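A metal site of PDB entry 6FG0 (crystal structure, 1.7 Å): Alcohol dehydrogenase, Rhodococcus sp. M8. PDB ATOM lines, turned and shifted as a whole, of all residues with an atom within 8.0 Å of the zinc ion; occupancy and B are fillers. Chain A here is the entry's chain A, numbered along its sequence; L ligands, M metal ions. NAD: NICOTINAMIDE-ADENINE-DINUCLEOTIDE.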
ATOM      1  N   GLY A  36     -10.683  27.724   4.588  1.00  0.00           N
ATOM      2  CA  GLY A  36     -11.433  26.508   4.968  1.00  0.00           C
ATOM      3  C   GLY A  36     -12.676  26.277   4.116  1.00  0.00           C
ATOM      4  O   GLY A  36     -13.339  27.213   3.720  1.00  0.00           O
ATOM      5  N   LEU A  37     -12.956  24.997   3.839  1.00  0.00           N
ATOM      6  CA  LEU A  37     -14.191  24.556   3.216  1.00  0.00           C
ATOM      7  C   LEU A  37     -15.139  24.168   4.339  1.00  0.00           C
ATOM      8  O   LEU A  37     -14.709  23.511   5.290  1.00  0.00           O
ATOM      9  CB  LEU A  37     -13.967  23.317   2.376  1.00  0.00           C
ATOM     10  CG  LEU A  37     -13.321  23.426   1.016  1.00  0.00           C
ATOM     11  CD1 LEU A  37     -11.820  23.658   1.100  1.00  0.00           C
ATOM     12  CD2 LEU A  37     -13.657  22.162   0.212  1.00  0.00           C
ATOM     13  N   CYS A  38     -16.408  24.533   4.205  1.00  0.00           N
ATOM     14  CA  CYS A  38     -17.441  24.210   5.197  1.00  0.00           C
ATOM     15  C   CYS A  38     -18.612  23.522   4.524  1.00  0.00           C
ATOM     16  O   CYS A  38     -18.951  23.847   3.390  1.00  0.00           O
ATOM     17  CB  CYS A  38     -17.928  25.475   5.881  1.00  0.00           C
ATOM     18  SG  CYS A  38     -19.215  25.214   7.166  1.00  0.00           S
ATOM     19  N   HIS A  39     -19.281  22.615   5.232  1.00  0.00           N
ATOM     20  CA  HIS A  39     -20.466  21.969   4.661  1.00  0.00           C
ATOM     21  C   HIS A  39     -21.572  22.975   4.313  1.00  0.00           C
ATOM     22  O   HIS A  39     -22.336  22.755   3.385  1.00  0.00           O
ATOM     23  CB  HIS A  39     -21.011  20.882   5.607  1.00  0.00           C
ATOM     24  CG  HIS A  39     -21.878  19.868   4.927  1.00  0.00           C
ATOM     25  ND1 HIS A  39     -21.487  18.560   4.768  1.00  0.00           N
ATOM     26  CD2 HIS A  39     -23.089  19.976   4.341  1.00  0.00           C
ATOM     27  CE1 HIS A  39     -22.440  17.896   4.121  1.00  0.00           C
ATOM     28  NE2 HIS A  39     -23.416  18.744   3.842  1.00  0.00           N
ATOM     29  N   SER A  40     -21.623  24.118   5.018  1.00  0.00           N
ATOM     30  CA  SER A  40     -22.567  25.199   4.643  1.00  0.00           C
ATOM     31  C   SER A  40     -22.407  25.625   3.180  1.00  0.00           C
ATOM     32  O   SER A  40     -23.377  26.023   2.535  1.00  0.00           O
ATOM     33  CB  SER A  40     -22.420  26.399   5.572  1.00  0.00           C
ATOM     34  OG  SER A  40     -22.836  26.056   6.871  1.00  0.00           O
ATOM     35  N   ASP A  41     -21.181  25.568   2.669  1.00  0.00           N
ATOM     36  CA  ASP A  41     -20.929  25.874   1.259  1.00  0.00           C
ATOM     37  C   ASP A  41     -21.691  24.944   0.305  1.00  0.00           C
ATOM     38  O   ASP A  41     -22.199  25.378  -0.726  1.00  0.00           O
ATOM     39  CB  ASP A  41     -19.430  25.766   0.936  1.00  0.00           C
ATOM     40  CG  ASP A  41     -18.583  26.776   1.684  1.00  0.00           C
ATOM     41  OD1 ASP A  41     -19.102  27.859   2.023  1.00  0.00           O
ATOM     42  OD2 ASP A  41     -17.392  26.501   1.921  1.00  0.00           O
ATOM     43  N   GLY A  61     -15.617  30.831   0.503  1.00  0.00           N
ATOM     44  CA  GLY A  61     -14.693  30.730   1.634  1.00  0.00           C
ATOM     45  C   GLY A  61     -15.016  31.685   2.747  1.00  0.00           C
ATOM     46  O   GLY A  61     -14.653  32.862   2.674  1.00  0.00           O
ATOM     47  N   HIS A  62     -15.669  31.199   3.778  1.00  0.00           N
ATOM     48  CA  HIS A  62     -15.942  32.028   4.944  1.00  0.00           C
ATOM     49  C   HIS A  62     -15.063  31.684   6.144  1.00  0.00           C
ATOM     50  O   HIS A  62     -15.272  32.224   7.243  1.00  0.00           O
ATOM     51  CB  HIS A  62     -17.431  32.018   5.288  1.00  0.00           C
ATOM     52  CG  HIS A  62     -17.998  30.661   5.493  1.00  0.00           C
ATOM     53  ND1 HIS A  62     -18.528  29.919   4.462  1.00  0.00           N
ATOM     54  CD2 HIS A  62     -18.130  29.904   6.613  1.00  0.00           C
ATOM     55  CE1 HIS A  62     -18.949  28.753   4.941  1.00  0.00           C
ATOM     56  NE2 HIS A  62     -18.745  28.740   6.249  1.00  0.00           N
ATOM     57  N   GLU A  63     -14.068  30.827   5.923  1.00  0.00           N
ATOM     58  CA  GLU A  63     -13.011  30.507   6.880  1.00  0.00           C
ATOM     59  C   GLU A  63     -11.692  31.007   6.306  1.00  0.00           C
ATOM     60  O   GLU A  63     -11.124  30.358   5.421  1.00  0.00           O
ATOM     61  CB  GLU A  63     -12.913  29.002   7.125  1.00  0.00           C
ATOM     62  CG  GLU A  63     -14.019  28.467   8.003  1.00  0.00           C
ATOM     63  CD  GLU A  63     -13.808  27.014   8.453  1.00  0.00           C
ATOM     64  OE1 GLU A  63     -12.972  26.266   7.886  1.00  0.00           O
ATOM     65  OE2 GLU A  63     -14.496  26.609   9.411  1.00  0.00           O
ATOM     66  N   THR A 152     -12.043  29.949  12.554  1.00  0.00           N
ATOM     67  CA  THR A 152     -12.996  31.021  12.255  1.00  0.00           C
ATOM     68  C   THR A 152     -14.448  30.575  12.100  1.00  0.00           C
ATOM     69  O   THR A 152     -15.332  31.416  12.037  1.00  0.00           O
ATOM     70  CB  THR A 152     -12.597  31.785  10.976  1.00  0.00           C
ATOM     71  OG1 THR A 152     -12.507  30.879   9.863  1.00  0.00           O
ATOM     72  CG2 THR A 152     -11.244  32.455  11.151  1.00  0.00           C
ATOM     73  N   ASP A 153     -14.690  29.273  12.022  1.00  0.00           N
ATOM     74  CA  ASP A 153     -16.061  28.756  11.928  1.00  0.00           C
ATOM     75  C   ASP A 153     -16.186  27.367  12.556  1.00  0.00           C
ATOM     76  O   ASP A 153     -16.984  27.198  13.495  1.00  0.00           O
ATOM     77  CB  ASP A 153     -16.505  28.821  10.476  1.00  0.00           C
ATOM     78  CG  ASP A 153     -17.963  28.427  10.265  1.00  0.00           C
ATOM     79  OD1 ASP A 153     -18.807  28.508  11.187  1.00  0.00           O
ATOM     80  OD2 ASP A 153     -18.261  28.036   9.138  1.00  0.00           O
ATOM     81  N   ALA A 154     -15.402  26.408  12.097  1.00  0.00           N
ATOM     82  CA  ALA A 154     -15.348  25.092  12.736  1.00  0.00           C
ATOM     83  C   ALA A 154     -15.011  25.209  14.215  1.00  0.00           C
ATOM     84  O   ALA A 154     -15.458  24.400  15.003  1.00  0.00           O
ATOM     85  CB  ALA A 154     -14.375  24.173  12.030  1.00  0.00           C
ATOM     86  N   THR A 157     -18.084  28.496  15.753  1.00  0.00           N
ATOM     87  CA  THR A 157     -19.489  28.126  15.847  1.00  0.00           C
ATOM     88  C   THR A 157     -19.775  27.168  17.027  1.00  0.00           C
ATOM     89  O   THR A 157     -20.637  27.453  17.848  1.00  0.00           O
ATOM     90  CB  THR A 157     -20.015  27.639  14.507  1.00  0.00           C
ATOM     91  OG1 THR A 157     -19.900  28.733  13.603  1.00  0.00           O
ATOM     92  CG2 THR A 157     -21.447  27.201  14.605  1.00  0.00           C
ATOM     93  N   LEU A 183     -16.872  20.804  12.287  1.00  0.00           N
ATOM     94  CA  LEU A 183     -17.306  21.440  13.523  1.00  0.00           C
ATOM     95  C   LEU A 183     -17.200  20.497  14.719  1.00  0.00           C
ATOM     96  O   LEU A 183     -16.649  20.864  15.766  1.00  0.00           O
ATOM     97  CB  LEU A 183     -18.751  21.965  13.425  1.00  0.00           C
ATOM     98  CG  LEU A 183     -18.910  23.383  12.904  1.00  0.00           C
ATOM     99  CD1 LEU A 183     -18.510  23.517  11.425  1.00  0.00           C
ATOM    100  CD2 LEU A 183     -20.326  23.866  13.135  1.00  0.00           C
ATOM    101  N   ILE A 271     -27.500  22.310   9.975  1.00  0.00           N
ATOM    102  CA  ILE A 271     -28.562  22.923   9.205  1.00  0.00           C
ATOM    103  C   ILE A 271     -29.069  21.925   8.155  1.00  0.00           C
ATOM    104  O   ILE A 271     -28.343  21.542   7.222  1.00  0.00           O
ATOM    105  CB  ILE A 271     -28.083  24.230   8.519  1.00  0.00           C
ATOM    106  CG1 ILE A 271     -27.631  25.252   9.591  1.00  0.00           C
ATOM    107  CG2 ILE A 271     -29.174  24.815   7.624  1.00  0.00           C
ATOM    108  CD1 ILE A 271     -26.784  26.409   9.049  1.00  0.00           C
ATOM    109  N   TRP A 295     -23.110  31.091  14.190  1.00  0.00           N
ATOM    110  CA  TRP A 295     -21.723  31.546  14.122  1.00  0.00           C
ATOM    111  C   TRP A 295     -21.218  31.915  15.532  1.00  0.00           C
ATOM    112  O   TRP A 295     -21.422  31.125  16.445  1.00  0.00           O
ATOM    113  CB  TRP A 295     -21.568  32.625  13.054  1.00  0.00           C
ATOM    114  CG  TRP A 295     -20.268  32.505  12.263  1.00  0.00           C
ATOM    115  CD1 TRP A 295     -19.092  32.002  12.694  1.00  0.00           C
ATOM    116  CD2 TRP A 295     -20.057  32.925  10.913  1.00  0.00           C
ATOM    117  NE1 TRP A 295     -18.147  32.062  11.680  1.00  0.00           N
ATOM    118  CE2 TRP A 295     -18.730  32.623  10.581  1.00  0.00           C
ATOM    119  CE3 TRP A 295     -20.879  33.518   9.951  1.00  0.00           C
ATOM    120  CZ2 TRP A 295     -18.192  32.885   9.323  1.00  0.00           C
ATOM    121  CZ3 TRP A 295     -20.349  33.795   8.725  1.00  0.00           C
ATOM    122  CH2 TRP A 295     -19.024  33.487   8.414  1.00  0.00           C
ATOM    123  N   ARG A 340     -11.283  18.914   8.489  1.00  0.00           N
ATOM    124  CA  ARG A 340     -11.522  20.098   7.672  1.00  0.00           C
ATOM    125  C   ARG A 340     -10.660  20.146   6.442  1.00  0.00           C
ATOM    126  O   ARG A 340      -9.428  19.971   6.512  1.00  0.00           O
ATOM    127  CB  ARG A 340     -11.249  21.383   8.468  1.00  0.00           C
ATOM    128  CG  ARG A 340     -12.506  22.077   8.947  1.00  0.00           C
ATOM    129  CD  ARG A 340     -13.180  22.773   7.803  1.00  0.00           C
ATOM    130  NE  ARG A 340     -14.193  23.725   8.256  1.00  0.00           N
ATOM    131  CZ  ARG A 340     -15.501  23.499   8.384  1.00  0.00           C
ATOM    132  NH1 ARG A 340     -16.036  22.292   8.171  1.00  0.00           N
ATOM    133  NH2 ARG A 340     -16.284  24.494   8.745  1.00  0.00           N
HETATM  134  PA  NAD L   1     -18.855  17.961   7.721  1.00  0.00           P
HETATM  135  O1A NAD L   1     -19.390  17.529   6.367  1.00  0.00           O
HETATM  136  O2A NAD L   1     -17.408  18.261   7.935  1.00  0.00           O
HETATM  137  O5B NAD L   1     -19.223  16.803   8.756  1.00  0.00           O
HETATM  138  C5B NAD L   1     -20.404  16.039   8.756  1.00  0.00           C
HETATM  139  C4B NAD L   1     -20.273  14.970   9.856  1.00  0.00           C
HETATM  140  O4B NAD L   1     -21.587  14.646  10.296  1.00  0.00           O
HETATM  141  C3B NAD L   1     -19.568  13.692   9.390  1.00  0.00           C
HETATM  142  O3B NAD L   1     -18.627  13.195  10.364  1.00  0.00           O
HETATM  143  C2B NAD L   1     -20.750  12.751   9.140  1.00  0.00           C
HETATM  144  O2B NAD L   1     -20.458  11.357   9.129  1.00  0.00           O
HETATM  145  C1B NAD L   1     -21.669  13.211  10.267  1.00  0.00           C
HETATM  146  N9A NAD L   1     -23.075  12.836  10.123  1.00  0.00           N
HETATM  147  C8A NAD L   1     -23.821  12.951   8.978  1.00  0.00           C
HETATM  148  N7A NAD L   1     -25.056  12.492   9.206  1.00  0.00           N
HETATM  149  C5A NAD L   1     -25.101  12.036  10.478  1.00  0.00           C
HETATM  150  C6A NAD L   1     -26.118  11.420  11.354  1.00  0.00           C
HETATM  151  N6A NAD L   1     -27.348  11.172  10.915  1.00  0.00           N
HETATM  152  N1A NAD L   1     -25.789  11.104  12.623  1.00  0.00           N
HETATM  153  C2A NAD L   1     -24.555  11.368  13.079  1.00  0.00           C
HETATM  154  N3A NAD L   1     -23.563  11.908  12.363  1.00  0.00           N
HETATM  155  C4A NAD L   1     -23.790  12.256  11.076  1.00  0.00           C
HETATM  156  O3  NAD L   1     -19.804  19.165   8.183  1.00  0.00           O
HETATM  157  PN  NAD L   1     -19.350  20.509   8.907  1.00  0.00           P
HETATM  158  O1N NAD L   1     -18.634  21.395   7.941  1.00  0.00           O
HETATM  159  O2N NAD L   1     -18.738  20.187  10.274  1.00  0.00           O
HETATM  160  O5D NAD L   1     -20.788  21.164   9.176  1.00  0.00           O
HETATM  161  C5D NAD L   1     -21.740  20.548  10.046  1.00  0.00           C
HETATM  162  C4D NAD L   1     -23.090  21.260   9.997  1.00  0.00           C
HETATM  163  O4D NAD L   1     -23.005  22.501  10.730  1.00  0.00           O
HETATM  164  C3D NAD L   1     -23.606  21.592   8.606  1.00  0.00           C
HETATM  165  O3D NAD L   1     -25.026  21.438   8.556  1.00  0.00           O
HETATM  166  C2D NAD L   1     -23.282  23.067   8.479  1.00  0.00           C
HETATM  167  O2D NAD L   1     -24.083  23.724   7.484  1.00  0.00           O
HETATM  168  C1D NAD L   1     -23.546  23.525   9.901  1.00  0.00           C
HETATM  169  N1N NAD L   1     -22.986  24.822  10.304  1.00  0.00           N
HETATM  170  C2N NAD L   1     -23.777  25.624  11.041  1.00  0.00           C
HETATM  171  C3N NAD L   1     -23.357  26.875  11.453  1.00  0.00           C
HETATM  172  C7N NAD L   1     -24.227  27.749  12.315  1.00  0.00           C
HETATM  173  O7N NAD L   1     -23.898  28.908  12.531  1.00  0.00           O
HETATM  174  N7N NAD L   1     -25.292  27.244  12.962  1.00  0.00           N
HETATM  175  C4N NAD L   1     -22.060  27.305  11.109  1.00  0.00           C
HETATM  176  C5N NAD L   1     -21.241  26.436  10.394  1.00  0.00           C
HETATM  177  C6N NAD L   1     -21.715  25.195  10.005  1.00  0.00           C
HETATM  178 ZN    ZN M   1     -19.409  27.456   7.712  1.00  0.00          ZN
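An oxygen (O2D) of the ligand sits at hydrogen-bond distance from the side-chain hydroxyl of Ser 40, at 2.7 Å. The guanidinium group of Arg 340 is in salt-bridge range of an oxygen (O1N) of the ligand (2.8 Å). N of His 39 is in hydrogen-bond range of O1N of the ligand, at 3.0 Å. An oxygen (O1A) of the ligand lies within hydrogen-bond range of a ring nitrogen (ND1) of His 39 (2.8 Å). O2N of the ligand lies within hydrogen-bond range of N of Leu 183, 2.8 Å away. The backbone NH (N) of Trp 295 sits at hydrogen-bond distance from an oxygen (O7N) of the ligand (2.9 Å). O3D of the ligand sits at hydrogen-bond distance from N of Ile 271 (3.0 Å).
OD1 of Asp 153 lies within hydrogen-bond range of OG1 of Thr 157 (2.7 Å). The side-chain carboxylate (OD1) of Asp 41 lies close to a ring nitrogen (ND1) of His 62 (3.2 Å). The backbone NH of Ser 40 lies close to the side-chain sulfur of Cys 38, at 3.4 Å. The guanidinium group of Arg 340 lies close to the side-chain sulfur of Cys 38 (3.4 Å). The backbone NH of Cys 38 lies within hydrogen-bond range of the side-chain carboxylate of Asp 41, 3.2 Å away.
Ser 40 touches the zinc ion. The nearest printed residue that does not touch the zinc ion is Arg 340 (4.4 Å).
The zinc ion is bound by OD2 of Asp 153, NE2 of His 62 and SG of Cys 38.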
